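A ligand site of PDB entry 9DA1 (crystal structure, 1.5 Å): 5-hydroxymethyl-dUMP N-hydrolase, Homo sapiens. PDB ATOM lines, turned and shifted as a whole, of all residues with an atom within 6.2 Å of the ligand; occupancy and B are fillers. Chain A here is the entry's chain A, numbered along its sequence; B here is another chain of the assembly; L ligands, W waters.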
ATOM      1  N   TYR A   7      18.374  -6.724   2.043  1.00  0.00           N
ATOM      2  CA  TYR A   7      19.166  -6.561   3.259  1.00  0.00           C
ATOM      3  C   TYR A   7      20.075  -5.371   3.016  1.00  0.00           C
ATOM      4  O   TYR A   7      20.800  -5.348   2.021  1.00  0.00           O
ATOM      5  CB  TYR A   7      20.030  -7.816   3.508  1.00  0.00           C
ATOM      6  CG  TYR A   7      20.788  -7.841   4.833  1.00  0.00           C
ATOM      7  CD1 TYR A   7      21.903  -7.045   5.039  1.00  0.00           C
ATOM      8  CD2 TYR A   7      20.365  -8.654   5.860  1.00  0.00           C
ATOM      9  CE1 TYR A   7      22.565  -7.031   6.281  1.00  0.00           C
ATOM     10  CE2 TYR A   7      21.024  -8.696   7.050  1.00  0.00           C
ATOM     11  CZ  TYR A   7      22.121  -7.877   7.266  1.00  0.00           C
ATOM     12  OH  TYR A   7      22.763  -7.939   8.489  1.00  0.00           O
ATOM     13  N   PHE A   8      20.011  -4.361   3.871  1.00  0.00           N
ATOM     14  CA  PHE A   8      20.860  -3.193   3.728  1.00  0.00           C
ATOM     15  C   PHE A   8      21.939  -3.163   4.789  1.00  0.00           C
ATOM     16  O   PHE A   8      21.659  -3.423   5.956  1.00  0.00           O
ATOM     17  CB  PHE A   8      20.038  -1.887   3.840  1.00  0.00           C
ATOM     18  CG  PHE A   8      20.923  -0.680   3.815  1.00  0.00           C
ATOM     19  CD1 PHE A   8      21.503  -0.269   2.625  1.00  0.00           C
ATOM     20  CD2 PHE A   8      21.269  -0.052   5.003  1.00  0.00           C
ATOM     21  CE1 PHE A   8      22.393   0.816   2.608  1.00  0.00           C
ATOM     22  CE2 PHE A   8      22.174   1.017   4.998  1.00  0.00           C
ATOM     23  CZ  PHE A   8      22.727   1.452   3.811  1.00  0.00           C
ATOM     24  N   CYS A   9      23.158  -2.813   4.358  1.00  0.00           N
ATOM     25  CA  CYS A   9      24.350  -2.703   5.202  1.00  0.00           C
ATOM     26  C   CYS A   9      24.932  -1.305   5.127  1.00  0.00           C
ATOM     27  O   CYS A   9      25.157  -0.775   4.046  1.00  0.00           O
ATOM     28  CB  CYS A   9      25.484  -3.711   4.886  1.00  0.00           C
ATOM     29  SG  CYS A   9      25.066  -5.299   4.304  1.00  0.00           S
ATOM     30  N   GLY A  10      25.199  -0.725   6.309  1.00  0.00           N
ATOM     31  CA  GLY A  10      25.904   0.539   6.396  1.00  0.00           C
ATOM     32  C   GLY A  10      26.481   0.705   7.774  1.00  0.00           C
ATOM     33  O   GLY A  10      25.933   0.192   8.742  1.00  0.00           O
ATOM     34  N   SER A  11      27.575   1.460   7.874  1.00  0.00           N
ATOM     35  CA  SER A  11      28.272   1.677   9.134  1.00  0.00           C
ATOM     36  C   SER A  11      27.371   2.201  10.244  1.00  0.00           C
ATOM     37  O   SER A  11      26.586   3.118  10.056  1.00  0.00           O
ATOM     38  CB  SER A  11      29.460   2.635   8.887  1.00  0.00           C
ATOM     39  OG  SER A  11      30.190   2.912  10.068  1.00  0.00           O
ATOM     40  N   ILE A  12      27.574   1.642  11.435  1.00  0.00           N
ATOM     41  CA  ILE A  12      26.953   2.162  12.649  1.00  0.00           C
ATOM     42  C   ILE A  12      28.064   2.466  13.646  1.00  0.00           C
ATOM     43  O   ILE A  12      28.424   3.634  13.834  1.00  0.00           O
ATOM     44  CB  ILE A  12      25.917   1.172  13.210  1.00  0.00           C
ATOM     45  CG1 ILE A  12      24.806   0.960  12.177  1.00  0.00           C
ATOM     46  CG2 ILE A  12      25.383   1.703  14.523  1.00  0.00           C
ATOM     47  CD1 ILE A  12      23.808  -0.112  12.510  1.00  0.00           C
ATOM     48  N   ARG A  13      28.660   1.442  14.278  1.00  0.00           N
ATOM     49  CA  ARG A  13      29.777   1.696  15.184  1.00  0.00           C
ATOM     50  C   ARG A  13      31.041   2.104  14.443  1.00  0.00           C
ATOM     51  O   ARG A  13      31.936   2.690  15.068  1.00  0.00           O
ATOM     52  CB  ARG A  13      30.021   0.506  16.100  1.00  0.00           C
ATOM     53  CG  ARG A  13      28.853   0.328  17.101  1.00  0.00           C
ATOM     54  CD  ARG A  13      29.042  -0.777  18.047  1.00  0.00           C
ATOM     55  NE  ARG A  13      27.860  -1.031  18.868  1.00  0.00           N
ATOM     56  CZ  ARG A  13      27.633  -2.145  19.542  1.00  0.00           C
ATOM     57  NH1 ARG A  13      28.565  -3.072  19.679  1.00  0.00           N
ATOM     58  NH2 ARG A  13      26.439  -2.341  20.090  1.00  0.00           N
ATOM     59  N   GLY A  14      31.141   1.859  13.139  1.00  0.00           N
ATOM     60  CA  GLY A  14      32.211   2.504  12.381  1.00  0.00           C
ATOM     61  C   GLY A  14      32.084   4.007  12.288  1.00  0.00           C
ATOM     62  O   GLY A  14      33.051   4.677  11.921  1.00  0.00           O
ATOM     63  N   GLY A  15      30.912   4.534  12.599  1.00  0.00           N
ATOM     64  CA  GLY A  15      30.615   5.936  12.475  1.00  0.00           C
ATOM     65  C   GLY A  15      29.338   6.121  11.680  1.00  0.00           C
ATOM     66  O   GLY A  15      29.040   5.331  10.770  1.00  0.00           O
ATOM     67  N   THR A  37      16.132  -5.649   7.168  1.00  0.00           N
ATOM     68  CA  THR A  37      16.911  -4.993   8.205  1.00  0.00           C
ATOM     69  C   THR A  37      16.235  -3.747   8.759  1.00  0.00           C
ATOM     70  O   THR A  37      16.816  -3.111   9.653  1.00  0.00           O
ATOM     71  CB  THR A  37      18.281  -4.661   7.608  1.00  0.00           C
ATOM     72  OG1 THR A  37      18.114  -4.028   6.337  1.00  0.00           O
ATOM     73  CG2 THR A  37      19.090  -5.958   7.418  1.00  0.00           C
ATOM     74  N   ASP A  56      24.924  -7.889  21.815  1.00  0.00           N
ATOM     75  CA  ASP A  56      25.513  -7.992  20.480  1.00  0.00           C
ATOM     76  C   ASP A  56      25.287  -9.375  19.871  1.00  0.00           C
ATOM     77  O   ASP A  56      25.182  -9.483  18.641  1.00  0.00           O
ATOM     78  CB  ASP A  56      27.002  -7.639  20.523  1.00  0.00           C
ATOM     79  CG  ASP A  56      27.246  -6.151  20.814  1.00  0.00           C
ATOM     80  OD1 ASP A  56      26.253  -5.388  20.883  1.00  0.00           O
ATOM     81  OD2 ASP A  56      28.418  -5.761  20.959  1.00  0.00           O
ATOM     82  N   ILE A  59      22.040  -9.273  18.035  1.00  0.00           N
ATOM     83  CA  ILE A  59      22.174  -8.518  16.782  1.00  0.00           C
ATOM     84  C   ILE A  59      22.808  -9.396  15.706  1.00  0.00           C
ATOM     85  O   ILE A  59      22.306  -9.479  14.576  1.00  0.00           O
ATOM     86  CB  ILE A  59      23.001  -7.241  17.006  1.00  0.00           C
ATOM     87  CG1 ILE A  59      22.232  -6.248  17.885  1.00  0.00           C
ATOM     88  CG2 ILE A  59      23.358  -6.626  15.657  1.00  0.00           C
ATOM     89  CD1 ILE A  59      23.051  -5.027  18.330  1.00  0.00           C
ATOM     90  N   ASP A  63      20.698 -10.678  12.439  1.00  0.00           N
ATOM     91  CA  ASP A  63      21.177 -10.213  11.142  1.00  0.00           C
ATOM     92  C   ASP A  63      21.544 -11.379  10.250  1.00  0.00           C
ATOM     93  O   ASP A  63      21.232 -11.370   9.048  1.00  0.00           O
ATOM     94  CB  ASP A  63      22.358  -9.283  11.335  1.00  0.00           C
ATOM     95  CG  ASP A  63      21.966  -7.913  11.818  1.00  0.00           C
ATOM     96  OD1 ASP A  63      20.787  -7.612  11.997  1.00  0.00           O
ATOM     97  OD2 ASP A  63      22.910  -7.084  12.045  1.00  0.00           O
ATOM     98  N   TRP A  66      18.456 -12.862   8.643  1.00  0.00           N
ATOM     99  CA  TRP A  66      17.958 -12.034   7.558  1.00  0.00           C
ATOM    100  C   TRP A  66      18.880 -12.091   6.348  1.00  0.00           C
ATOM    101  O   TRP A  66      18.419 -12.086   5.198  1.00  0.00           O
ATOM    102  CB  TRP A  66      17.814 -10.594   8.038  1.00  0.00           C
ATOM    103  CG  TRP A  66      16.727 -10.383   9.013  1.00  0.00           C
ATOM    104  CD1 TRP A  66      15.549 -11.007   9.061  1.00  0.00           C
ATOM    105  CD2 TRP A  66      16.726  -9.408  10.053  1.00  0.00           C
ATOM    106  NE1 TRP A  66      14.772 -10.505  10.082  1.00  0.00           N
ATOM    107  CE2 TRP A  66      15.494  -9.522  10.718  1.00  0.00           C
ATOM    108  CE3 TRP A  66      17.643  -8.448  10.485  1.00  0.00           C
ATOM    109  CZ2 TRP A  66      15.155  -8.722  11.807  1.00  0.00           C
ATOM    110  CZ3 TRP A  66      17.300  -7.654  11.562  1.00  0.00           C
ATOM    111  CH2 TRP A  66      16.074  -7.797  12.216  1.00  0.00           C
ATOM    112  N   PRO A  80      34.350   3.207   6.409  1.00  0.00           N
ATOM    113  CA  PRO A  80      34.892   1.905   6.800  1.00  0.00           C
ATOM    114  C   PRO A  80      34.206   1.357   8.035  1.00  0.00           C
ATOM    115  O   PRO A  80      33.950   2.076   8.998  1.00  0.00           O
ATOM    116  CB  PRO A  80      36.375   2.194   7.075  1.00  0.00           C
ATOM    117  CG  PRO A  80      36.670   3.378   6.220  1.00  0.00           C
ATOM    118  CD  PRO A  80      35.413   4.222   6.255  1.00  0.00           C
ATOM    119  N   SER A  81      33.944   0.056   8.025  1.00  0.00           N
ATOM    120  CA  SER A  81      33.183  -0.589   9.086  1.00  0.00           C
ATOM    121  C   SER A  81      33.468  -2.075   9.134  1.00  0.00           C
ATOM    122  O   SER A  81      33.354  -2.751   8.117  1.00  0.00           O
ATOM    123  CB  SER A  81      31.689  -0.387   8.783  1.00  0.00           C
ATOM    124  OG  SER A  81      30.866  -1.309   9.505  1.00  0.00           O
ATOM    125  N   LEU A  82      33.780  -2.582  10.328  1.00  0.00           N
ATOM    126  CA  LEU A  82      33.992  -4.009  10.485  1.00  0.00           C
ATOM    127  C   LEU A  82      32.719  -4.779  10.191  1.00  0.00           C
ATOM    128  O   LEU A  82      32.754  -5.829   9.537  1.00  0.00           O
ATOM    129  CB  LEU A  82      34.454  -4.349  11.899  1.00  0.00           C
ATOM    130  CG  LEU A  82      35.820  -3.811  12.301  1.00  0.00           C
ATOM    131  CD1 LEU A  82      35.952  -3.920  13.796  1.00  0.00           C
ATOM    132  CD2 LEU A  82      36.928  -4.552  11.616  1.00  0.00           C
ATOM    133  N   GLY A  83      31.590  -4.278  10.679  1.00  0.00           N
ATOM    134  CA  GLY A  83      30.345  -5.023  10.572  1.00  0.00           C
ATOM    135  C   GLY A  83      29.869  -5.108   9.132  1.00  0.00           C
ATOM    136  O   GLY A  83      29.369  -6.160   8.707  1.00  0.00           O
ATOM    137  N   VAL A  84      30.003  -4.034   8.375  1.00  0.00           N
ATOM    138  CA  VAL A  84      29.655  -4.085   6.974  1.00  0.00           C
ATOM    139  C   VAL A  84      30.547  -5.064   6.233  1.00  0.00           C
ATOM    140  O   VAL A  84      30.081  -5.856   5.414  1.00  0.00           O
ATOM    141  CB  VAL A  84      29.701  -2.687   6.352  1.00  0.00           C
ATOM    142  CG1 VAL A  84      29.476  -2.731   4.822  1.00  0.00           C
ATOM    143  CG2 VAL A  84      28.649  -1.761   6.965  1.00  0.00           C
ATOM    144  N   GLU A  87      29.450  -8.624   7.194  1.00  0.00           N
ATOM    145  CA  GLU A  87      28.219  -8.971   6.488  1.00  0.00           C
ATOM    146  C   GLU A  87      28.499  -9.337   5.031  1.00  0.00           C
ATOM    147  O   GLU A  87      27.971 -10.308   4.509  1.00  0.00           O
ATOM    148  CB  GLU A  87      27.177  -7.846   6.555  1.00  0.00           C
ATOM    149  CG  GLU A  87      26.714  -7.530   7.957  1.00  0.00           C
ATOM    150  CD  GLU A  87      25.820  -6.280   8.024  1.00  0.00           C
ATOM    151  OE1 GLU A  87      26.210  -5.200   7.617  1.00  0.00           O
ATOM    152  OE2 GLU A  87      24.806  -6.398   8.788  1.00  0.00           O
ATOM    153  N   LEU B 110      33.315  -1.661  20.084  1.00  0.00           N
ATOM    154  CA  LEU B 110      33.554  -2.606  18.999  1.00  0.00           C
ATOM    155  C   LEU B 110      32.240  -3.022  18.351  1.00  0.00           C
ATOM    156  O   LEU B 110      31.250  -3.320  19.032  1.00  0.00           O
ATOM    157  CB  LEU B 110      34.277  -3.837  19.544  1.00  0.00           C
ATOM    158  CG  LEU B 110      34.491  -4.971  18.558  1.00  0.00           C
ATOM    159  CD1 LEU B 110      35.365  -4.574  17.421  1.00  0.00           C
ATOM    160  CD2 LEU B 110      35.094  -6.146  19.330  1.00  0.00           C
ATOM    161  N   SER B 111      32.251  -3.058  17.026  1.00  0.00           N
ATOM    162  CA  SER B 111      31.169  -3.629  16.235  1.00  0.00           C
ATOM    163  C   SER B 111      30.443  -4.797  16.887  1.00  0.00           C
ATOM    164  O   SER B 111      31.061  -5.795  17.276  1.00  0.00           O
ATOM    165  CB  SER B 111      31.767  -4.131  14.927  1.00  0.00           C
ATOM    166  OG  SER B 111      30.779  -4.656  14.063  1.00  0.00           O
ATOM    167  N   ALA B 112      29.121  -4.693  16.911  1.00  0.00           N
ATOM    168  CA  ALA B 112      28.303  -5.816  17.381  1.00  0.00           C
ATOM    169  C   ALA B 112      28.477  -7.060  16.520  1.00  0.00           C
ATOM    170  O   ALA B 112      28.270  -8.182  16.999  1.00  0.00           O
ATOM    171  CB  ALA B 112      26.821  -5.465  17.396  1.00  0.00           C
ATOM    172  N   MET B 113      28.813  -6.906  15.225  1.00  0.00           N
ATOM    173  CA  MET B 113      28.942  -8.087  14.394  1.00  0.00           C
ATOM    174  C   MET B 113      30.175  -8.879  14.769  1.00  0.00           C
ATOM    175  O   MET B 113      30.217 -10.101  14.580  1.00  0.00           O
ATOM    176  CB  MET B 113      29.010  -7.660  12.925  1.00  0.00           C
ATOM    177  CG  MET B 113      27.801  -6.913  12.484  1.00  0.00           C
ATOM    178  SD  MET B 113      26.212  -7.711  12.824  1.00  0.00           S
ATOM    179  CE  MET B 113      26.279  -9.092  11.712  1.00  0.00           C
HETATM  180  N1  LIG L   1      24.596  -3.892  12.920  1.00  0.00           N
HETATM  181  C1  LIG L   1      23.252  -3.921  13.372  1.00  0.00           C
HETATM  182  O1  LIG L   1      22.415  -4.435  12.688  1.00  0.00           O
HETATM  183  N2  LIG L   1      22.933  -3.294  14.569  1.00  0.00           N
HETATM  184  C2  LIG L   1      23.892  -2.709  15.366  1.00  0.00           C
HETATM  185  O2  LIG L   1      23.606  -2.185  16.416  1.00  0.00           O
HETATM  186  C3  LIG L   1      25.329  -2.755  14.934  1.00  0.00           C
HETATM  187  C4  LIG L   1      25.640  -3.317  13.770  1.00  0.00           C
HETATM  188  C5  LIG L   1      24.866  -4.428  11.637  1.00  0.00           C
HETATM  189  C6  LIG L   1      24.182  -3.586  10.572  1.00  0.00           C
HETATM  190  C7  LIG L   1      25.183  -2.783   9.824  1.00  0.00           C
HETATM  191  C8  LIG L   1      26.530  -3.218  10.332  1.00  0.00           C
HETATM  192  C9  LIG L   1      27.249  -2.078  11.024  1.00  0.00           C
HETATM  193  C10 LIG L   1      26.355  -2.149  15.841  1.00  0.00           C
HETATM  194  O3  LIG L   1      28.490  -1.236  13.702  1.00  0.00           O
HETATM  195  O4  LIG L   1      23.459  -4.426   9.662  1.00  0.00           O
HETATM  196  O5  LIG L   1      25.144  -2.898   8.391  1.00  0.00           O
HETATM  197  O6  LIG L   1      26.291  -4.288  11.306  1.00  0.00           O
HETATM  198  O7  LIG L   1      28.501  -2.509  11.535  1.00  0.00           O
HETATM  199  O8  LIG L   1      27.646  -2.691  15.574  1.00  0.00           O
HETATM  200  O9  LIG L   1      30.614  -2.365  12.755  1.00  0.00           O
HETATM  201  O10 LIG L   1      29.670  -0.318  11.699  1.00  0.00           O
HETATM  202  P1  LIG L   1      29.392  -1.560  12.463  1.00  0.00           P
HETATM  203  O   HOH W   1      20.341  -3.612  15.292  1.00  0.00           O
HETATM  204  O   HOH W   2      21.352  -2.024  18.362  1.00  0.00           O
HETATM  205  O   HOH W   3      21.911  -2.394   8.400  1.00  0.00           O
HETATM  206  O   HOH W   4      33.125  -1.134  12.753  1.00  0.00           O
HETATM  207  O   HOH W   5      20.582  -5.159  10.198  1.00  0.00           O
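The side-chain carboxylate (OE2) of Glu 87 lies within hydrogen-bond range of an oxygen (O4) of the ligand (2.5 Å). An oxygen (O9) of the ligand lies within hydrogen-bond range of the side-chain hydroxyl of Ser 111 of chain B (2.6 Å). OG of Ser 81 lies within hydrogen-bond range of O10 of the ligand (2.7 Å). N of Arg 13 lies within hydrogen-bond range of O3 of the ligand (2.7 Å). The backbone NH of Ala 112 of chain B sits at hydrogen-bond distance from an oxygen (O8) of the ligand, at 2.8 Å. N of Ile 12 is in hydrogen-bond range of O10 of the ligand. The backbone NH (N) of Gly 83 is in hydrogen-bond range of an oxygen (O9) of the ligand (3.0 Å). N of Gly 14 is in hydrogen-bond range of O10 of the ligand (3.0 Å). O5 of the ligand lies within hydrogen-bond range of N of Gly 10 (3.0 Å). O of Gly 10 lies within hydrogen-bond range of O5 of the ligand, at 3.2 Å.
The side-chain carboxylate of Glu 87 lies close to the side-chain sulfur of Cys 9, at 3.5 Å. OE2 of Glu 87 sits at hydrogen-bond distance from OH of Tyr 7, 2.6 Å away. N of Met 113 of chain B lies close to OG of Ser 111 of chain B (3.2 Å). OG of Ser 81 sits at hydrogen-bond distance from N of Gly 83. N of Val 84 sits at hydrogen-bond distance from OG of Ser 81, at 3.1 Å. NH1 of Arg 13 is in hydrogen-bond range of O of Leu 110 of chain B (2.8 Å). The guanidinium group (NH1) of Arg 13 lies within salt-bridge range of the side-chain carboxylate (OD2) of Asp 56. O of Gly 15 is in hydrogen-bond range of OG of Ser 11, at 2.8 Å.
Water W4 bridges an oxygen (O9) of the ligand (2.8 Å) and the backbone NH of Leu 82 (2.9 Å). Water W3 lies within hydrogen-bond range of the backbone carbonyl oxygen (O) of Phe 8 (2.7 Å) and an oxygen (O4) of the ligand (2.8 Å). Water W5 bridges O4 of the ligand (3.0 Å) and OD1 of Asp 63 (3.0 Å).
An oxygen (O1) of the ligand sits close to the side-chain carboxylate (OD2) of Asp 63. An oxygen (O6) of the ligand sits close to the side-chain sulfur (SD) of Met 113 of chain B, at 3.7 Å. Residues that only touch the ligand: Tyr 7, Cys 9, Ser 11, Ile 59, Leu 82 and Val 84. Hydrophobic or aromatic side chains within 4 Å of the ligand: Ile 12, Ile 59, Val 84, Ala 112 of chain B and Met 113 of chain B. Of the 24 residues printed, 17 come within 4 Å of the ligand. The nearest printed residue that does not touch the ligand is Phe 8 (4.2 Å).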
